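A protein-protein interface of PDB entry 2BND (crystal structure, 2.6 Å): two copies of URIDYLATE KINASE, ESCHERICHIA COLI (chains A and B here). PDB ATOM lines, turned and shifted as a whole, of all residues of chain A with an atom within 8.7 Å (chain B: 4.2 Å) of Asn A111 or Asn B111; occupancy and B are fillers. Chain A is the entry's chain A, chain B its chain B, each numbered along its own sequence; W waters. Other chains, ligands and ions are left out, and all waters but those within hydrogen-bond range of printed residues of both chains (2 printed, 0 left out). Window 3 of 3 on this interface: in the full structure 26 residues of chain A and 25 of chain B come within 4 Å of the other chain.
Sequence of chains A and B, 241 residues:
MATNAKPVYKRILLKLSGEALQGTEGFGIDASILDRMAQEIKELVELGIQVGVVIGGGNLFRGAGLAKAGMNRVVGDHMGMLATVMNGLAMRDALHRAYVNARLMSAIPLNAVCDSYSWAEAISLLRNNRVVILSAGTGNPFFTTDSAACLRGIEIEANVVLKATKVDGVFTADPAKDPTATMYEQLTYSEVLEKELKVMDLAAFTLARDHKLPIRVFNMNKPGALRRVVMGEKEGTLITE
Pro B109 touches its own counterpart, Pro A109. Pro A109 touches Leu B110, and with the chains exchanged Leu A110 touches Pro B109. Pro A109 touches Asn B111, and with the chains exchanged Asn A111 touches Pro B109. Leu A110 touches its own counterpart, Leu B110. Of the 9 pairs that touch across the chains among the printed residues, 7 have their exchanged pair printed and touching as well.
Of the 13 printed residues of chain A, 5 touch a printed residue of chain B. Hydrophobic or aromatic side chains of chain A within 4 Å of the printed part of chain B: Leu A82, Ile A108, Pro A109 and Leu A110. Hydrophobic or aromatic side chains of chain B that line the printed part of chain A: Leu B110 and Val B113. Along chain B the printed residues that touch a printed residue of chain A span positions 109 to 113. Among the printed residues, no Asp or Glu carboxylate lies within 4 Å of a Lys or Arg side-chain nitrogen of the other chain.
CD1 of Leu B110 touches CD2 of Leu A82, at 3.6 Å. CG2 of Val B113 touches CG2 of Ile A108 (3.5 Å). O of Pro B109 touches O of Pro A109 (3.8 Å). O of Pro A109 touches ND2 of Asn B111, 3.7 Å away. Leu A110 touches Pro B109 (CA to O, 3.7 Å). Leu A110 touches Leu B110.
The backbone NH (N) of Asn A111 lies within hydrogen-bond range of the backbone carbonyl oxygen (O) of Pro B109 (3.4 Å). The side-chain amide oxygen (OD1) of Asn A111 lies within hydrogen-bond range of the side-chain amide nitrogen (ND2) of Asn B111, 2.9 Å away. The backbone carbonyl oxygen (O) of Pro A109 lies close to the backbone carbonyl oxygen (O) of Leu B110, 2.3 Å away.
OG of Ser A106 sits at hydrogen-bond distance from O of Ile A108, 2.6 Å away. OG of Ser B116 is in hydrogen-bond range of OD1 of Asn B111.
Of the printed residues of chain B, Asn A111 touches Pro B109 (3.4 Å) and Asn B111 (2.9 Å). Asn B111 touches just these residues of chain A: Pro A109 (3.7 Å) and Asn A111 (2.9 Å). Of the printed residues of chain B, Leu A110 touches Pro B109 and Leu B110. Of the printed residues of chain B, Ile A108 touches Val B113 (3.5 Å). Of the printed residues of chain A, Val B113 touches Ile A108. Printed residues of chain A within 4 Å of Pro B109: Pro A109 (3.8 Å), Leu A110 (3.7 Å) and Asn A111 (3.4 Å). His A78 touches none of the printed residues of chain B. The nearest residue of chain A that does not touch Asn B111 is Ile A108 (4.5 Å).
Water W1 lies within hydrogen-bond range of the backbone carbonyl oxygen of Val B113 (2.6 Å) and a ring nitrogen (ND1) of His A78 (3.0 Å). Water W2 bridges O of Ala B112 (3.1 Å) and NE2 of His A78 (3.5 Å).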
ATOM      1  N   HIS A  78      -1.879  -9.030  -0.928  1.00  0.00           N
ATOM      2  CA  HIS A  78      -1.904  -9.793   0.305  1.00  0.00           C
ATOM      3  C   HIS A  78      -0.584  -9.535   1.032  1.00  0.00           C
ATOM      4  O   HIS A  78      -0.570  -9.082   2.170  1.00  0.00           O
ATOM      5  CB  HIS A  78      -2.099 -11.291   0.013  1.00  0.00           C
ATOM      6  CG  HIS A  78      -3.531 -11.690  -0.189  1.00  0.00           C
ATOM      7  ND1 HIS A  78      -3.903 -12.958  -0.583  1.00  0.00           N
ATOM      8  CD2 HIS A  78      -4.681 -10.985  -0.066  1.00  0.00           C
ATOM      9  CE1 HIS A  78      -5.219 -13.014  -0.697  1.00  0.00           C
ATOM     10  NE2 HIS A  78      -5.715 -11.830  -0.390  1.00  0.00           N
ATOM     11  N   LEU A  82       0.196  -7.963   4.661  1.00  0.00           N
ATOM     12  CA  LEU A  82       0.992  -8.582   5.706  1.00  0.00           C
ATOM     13  C   LEU A  82       2.055  -7.604   6.141  1.00  0.00           C
ATOM     14  O   LEU A  82       2.449  -7.589   7.302  1.00  0.00           O
ATOM     15  CB  LEU A  82       1.658  -9.872   5.218  1.00  0.00           C
ATOM     16  CG  LEU A  82       0.791 -11.126   5.093  1.00  0.00           C
ATOM     17  CD1 LEU A  82       1.693 -12.330   4.817  1.00  0.00           C
ATOM     18  CD2 LEU A  82      -0.008 -11.357   6.374  1.00  0.00           C
ATOM     19  N   SER A 106      -5.652  -7.039  13.559  1.00  0.00           N
ATOM     20  CA  SER A 106      -5.452  -7.190  12.128  1.00  0.00           C
ATOM     21  C   SER A 106      -6.721  -7.581  11.386  1.00  0.00           C
ATOM     22  O   SER A 106      -7.481  -8.434  11.847  1.00  0.00           O
ATOM     23  CB  SER A 106      -4.359  -8.225  11.838  1.00  0.00           C
ATOM     24  OG  SER A 106      -4.345  -8.549  10.452  1.00  0.00           O
ATOM     25  N   ALA A 107      -6.932  -6.943  10.235  1.00  0.00           N
ATOM     26  CA  ALA A 107      -8.087  -7.216   9.387  1.00  0.00           C
ATOM     27  C   ALA A 107      -7.943  -8.646   8.876  1.00  0.00           C
ATOM     28  O   ALA A 107      -8.923  -9.320   8.580  1.00  0.00           O
ATOM     29  CB  ALA A 107      -8.121  -6.239   8.222  1.00  0.00           C
ATOM     30  N   ILE A 108      -6.698  -9.094   8.774  1.00  0.00           N
ATOM     31  CA  ILE A 108      -6.393 -10.436   8.325  1.00  0.00           C
ATOM     32  C   ILE A 108      -6.035 -11.216   9.581  1.00  0.00           C
ATOM     33  O   ILE A 108      -4.925 -11.098  10.096  1.00  0.00           O
ATOM     34  CB  ILE A 108      -5.207 -10.427   7.330  1.00  0.00           C
ATOM     35  CG1 ILE A 108      -5.672  -9.844   5.996  1.00  0.00           C
ATOM     36  CG2 ILE A 108      -4.662 -11.827   7.126  1.00  0.00           C
ATOM     37  CD1 ILE A 108      -4.677  -9.994   4.868  1.00  0.00           C
ATOM     38  N   PRO A 109      -6.983 -12.025  10.089  1.00  0.00           N
ATOM     39  CA  PRO A 109      -6.847 -12.858  11.293  1.00  0.00           C
ATOM     40  C   PRO A 109      -5.454 -13.460  11.398  1.00  0.00           C
ATOM     41  O   PRO A 109      -5.074 -14.273  10.563  1.00  0.00           O
ATOM     42  CB  PRO A 109      -7.916 -13.922  11.095  1.00  0.00           C
ATOM     43  CG  PRO A 109      -8.996 -13.174  10.354  1.00  0.00           C
ATOM     44  CD  PRO A 109      -8.208 -12.377   9.342  1.00  0.00           C
ATOM     45  N   LEU A 110      -4.702 -13.068  12.424  1.00  0.00           N
ATOM     46  CA  LEU A 110      -3.338 -13.549  12.602  1.00  0.00           C
ATOM     47  C   LEU A 110      -3.080 -14.047  14.020  1.00  0.00           C
ATOM     48  O   LEU A 110      -2.226 -13.521  14.744  1.00  0.00           O
ATOM     49  CB  LEU A 110      -2.359 -12.427  12.260  1.00  0.00           C
ATOM     50  CG  LEU A 110      -0.873 -12.779  12.279  1.00  0.00           C
ATOM     51  CD1 LEU A 110      -0.599 -13.835  11.234  1.00  0.00           C
ATOM     52  CD2 LEU A 110      -0.041 -11.536  12.013  1.00  0.00           C
ATOM     53  N   ASN A 111      -3.823 -15.077  14.403  1.00  0.00           N
ATOM     54  CA  ASN A 111      -3.719 -15.683  15.724  1.00  0.00           C
ATOM     55  C   ASN A 111      -2.278 -15.798  16.228  1.00  0.00           C
ATOM     56  O   ASN A 111      -1.390 -16.220  15.484  1.00  0.00           O
ATOM     57  CB  ASN A 111      -4.359 -17.070  15.685  1.00  0.00           C
ATOM     58  CG  ASN A 111      -5.711 -17.063  14.990  1.00  0.00           C
ATOM     59  OD1 ASN A 111      -5.846 -16.556  13.870  1.00  0.00           O
ATOM     60  ND2 ASN A 111      -6.718 -17.638  15.645  1.00  0.00           N
ATOM     61  N   ALA A 112      -2.074 -15.415  17.494  1.00  0.00           N
ATOM     62  CA  ALA A 112      -0.776 -15.465  18.185  1.00  0.00           C
ATOM     63  C   ALA A 112      -0.018 -14.133  18.240  1.00  0.00           C
ATOM     64  O   ALA A 112       0.244 -13.601  19.323  1.00  0.00           O
ATOM     65  CB  ALA A 112       0.130 -16.552  17.569  1.00  0.00           C
ATOM     66  N   VAL A 113       0.340 -13.606  17.071  1.00  0.00           N
ATOM     67  CA  VAL A 113       1.076 -12.348  16.985  1.00  0.00           C
ATOM     68  C   VAL A 113       0.249 -11.189  17.530  1.00  0.00           C
ATOM     69  O   VAL A 113       0.756 -10.325  18.238  1.00  0.00           O
ATOM     70  CB  VAL A 113       1.472 -12.057  15.534  1.00  0.00           C
ATOM     71  CG1 VAL A 113       2.451 -10.910  15.485  1.00  0.00           C
ATOM     72  CG2 VAL A 113       2.080 -13.297  14.918  1.00  0.00           C
ATOM     73  N   CYS A 114      -1.033 -11.184  17.195  1.00  0.00           N
ATOM     74  CA  CYS A 114      -1.945 -10.149  17.660  1.00  0.00           C
ATOM     75  C   CYS A 114      -3.347 -10.730  17.569  1.00  0.00           C
ATOM     76  O   CYS A 114      -3.505 -11.891  17.191  1.00  0.00           O
ATOM     77  CB  CYS A 114      -1.833  -8.906  16.771  1.00  0.00           C
ATOM     78  SG  CYS A 114      -2.057  -9.208  14.988  1.00  0.00           S
ATOM     79  N   ASP A 115      -4.359  -9.950  17.938  1.00  0.00           N
ATOM     80  CA  ASP A 115      -5.725 -10.438  17.822  1.00  0.00           C
ATOM     81  C   ASP A 115      -6.318  -9.867  16.541  1.00  0.00           C
ATOM     82  O   ASP A 115      -5.727  -8.993  15.912  1.00  0.00           O
ATOM     83  CB  ASP A 115      -6.594 -10.051  19.031  1.00  0.00           C
ATOM     84  CG  ASP A 115      -5.952  -9.009  19.925  1.00  0.00           C
ATOM     85  OD1 ASP A 115      -4.956  -9.326  20.618  1.00  0.00           O
ATOM     86  OD2 ASP A 115      -6.458  -7.870  19.940  1.00  0.00           O
ATOM     87  N   SER A 116      -7.476 -10.373  16.143  1.00  0.00           N
ATOM     88  CA  SER A 116      -8.110  -9.899  14.923  1.00  0.00           C
ATOM     89  C   SER A 116      -8.962  -8.667  15.168  1.00  0.00           C
ATOM     90  O   SER A 116      -9.486  -8.461  16.268  1.00  0.00           O
ATOM     91  CB  SER A 116      -8.948 -11.015  14.310  1.00  0.00           C
ATOM     92  OG  SER A 116      -9.608 -11.741  15.319  1.00  0.00           O
ATOM     93  N   PRO B 109      -1.164 -19.577  12.483  1.00  0.00           N
ATOM     94  CA  PRO B 109      -2.400 -19.459  11.699  1.00  0.00           C
ATOM     95  C   PRO B 109      -2.714 -18.077  11.140  1.00  0.00           C
ATOM     96  O   PRO B 109      -2.978 -17.137  11.886  1.00  0.00           O
ATOM     97  CB  PRO B 109      -3.473 -19.945  12.668  1.00  0.00           C
ATOM     98  CG  PRO B 109      -2.741 -20.962  13.489  1.00  0.00           C
ATOM     99  CD  PRO B 109      -1.421 -20.262  13.762  1.00  0.00           C
ATOM    100  N   LEU B 110      -2.686 -17.978   9.813  1.00  0.00           N
ATOM    101  CA  LEU B 110      -2.984 -16.746   9.099  1.00  0.00           C
ATOM    102  C   LEU B 110      -4.440 -16.795   8.681  1.00  0.00           C
ATOM    103  O   LEU B 110      -5.169 -15.808   8.793  1.00  0.00           O
ATOM    104  CB  LEU B 110      -2.117 -16.631   7.847  1.00  0.00           C
ATOM    105  CG  LEU B 110      -0.845 -15.796   7.948  1.00  0.00           C
ATOM    106  CD1 LEU B 110      -1.223 -14.326   8.092  1.00  0.00           C
ATOM    107  CD2 LEU B 110       0.002 -16.282   9.123  1.00  0.00           C
ATOM    108  N   ASN B 111      -4.855 -17.955   8.184  1.00  0.00           N
ATOM    109  CA  ASN B 111      -6.231 -18.152   7.754  1.00  0.00           C
ATOM    110  C   ASN B 111      -6.582 -17.168   6.639  1.00  0.00           C
ATOM    111  O   ASN B 111      -6.313 -15.966   6.743  1.00  0.00           O
ATOM    112  CB  ASN B 111      -7.158 -17.966   8.952  1.00  0.00           C
ATOM    113  CG  ASN B 111      -6.527 -18.456  10.244  1.00  0.00           C
ATOM    114  OD1 ASN B 111      -6.066 -19.596  10.325  1.00  0.00           O
ATOM    115  ND2 ASN B 111      -6.496 -17.590  11.262  1.00  0.00           N
ATOM    116  N   ALA B 112      -7.178 -17.693   5.571  1.00  0.00           N
ATOM    117  CA  ALA B 112      -7.566 -16.901   4.409  1.00  0.00           C
ATOM    118  C   ALA B 112      -6.373 -16.690   3.474  1.00  0.00           C
ATOM    119  O   ALA B 112      -6.390 -17.146   2.329  1.00  0.00           O
ATOM    120  CB  ALA B 112      -8.149 -15.558   4.848  1.00  0.00           C
ATOM    121  N   VAL B 113      -5.339 -16.004   3.957  1.00  0.00           N
ATOM    122  CA  VAL B 113      -4.145 -15.753   3.152  1.00  0.00           C
ATOM    123  C   VAL B 113      -3.470 -17.079   2.789  1.00  0.00           C
ATOM    124  O   VAL B 113      -3.004 -17.264   1.663  1.00  0.00           O
ATOM    125  CB  VAL B 113      -3.146 -14.858   3.908  1.00  0.00           C
ATOM    126  CG1 VAL B 113      -1.903 -14.643   3.074  1.00  0.00           C
ATOM    127  CG2 VAL B 113      -3.794 -13.525   4.228  1.00  0.00           C
ATOM    128  N   CYS B 114      -3.413 -17.998   3.749  1.00  0.00           N
ATOM    129  CA  CYS B 114      -2.829 -19.315   3.516  1.00  0.00           C
ATOM    130  C   CYS B 114      -3.398 -20.291   4.541  1.00  0.00           C
ATOM    131  O   CYS B 114      -4.206 -19.903   5.372  1.00  0.00           O
ATOM    132  CB  CYS B 114      -1.298 -19.265   3.615  1.00  0.00           C
ATOM    133  SG  CYS B 114      -0.637 -18.800   5.236  1.00  0.00           S
ATOM    134  N   SER B 116      -3.197 -23.209   7.721  1.00  0.00           N
ATOM    135  CA  SER B 116      -2.477 -23.396   8.974  1.00  0.00           C
ATOM    136  C   SER B 116      -1.688 -24.678   8.751  1.00  0.00           C
ATOM    137  O   SER B 116      -2.122 -25.534   7.984  1.00  0.00           O
ATOM    138  CB  SER B 116      -3.455 -23.605  10.127  1.00  0.00           C
ATOM    139  OG  SER B 116      -4.457 -22.606  10.136  1.00  0.00           O
HETATM  140  O   HOH W   1      -3.337 -15.923  -0.506  1.00  0.00           O
HETATM  141  O   HOH W   2      -7.360 -14.600   0.870  1.00  0.00           O
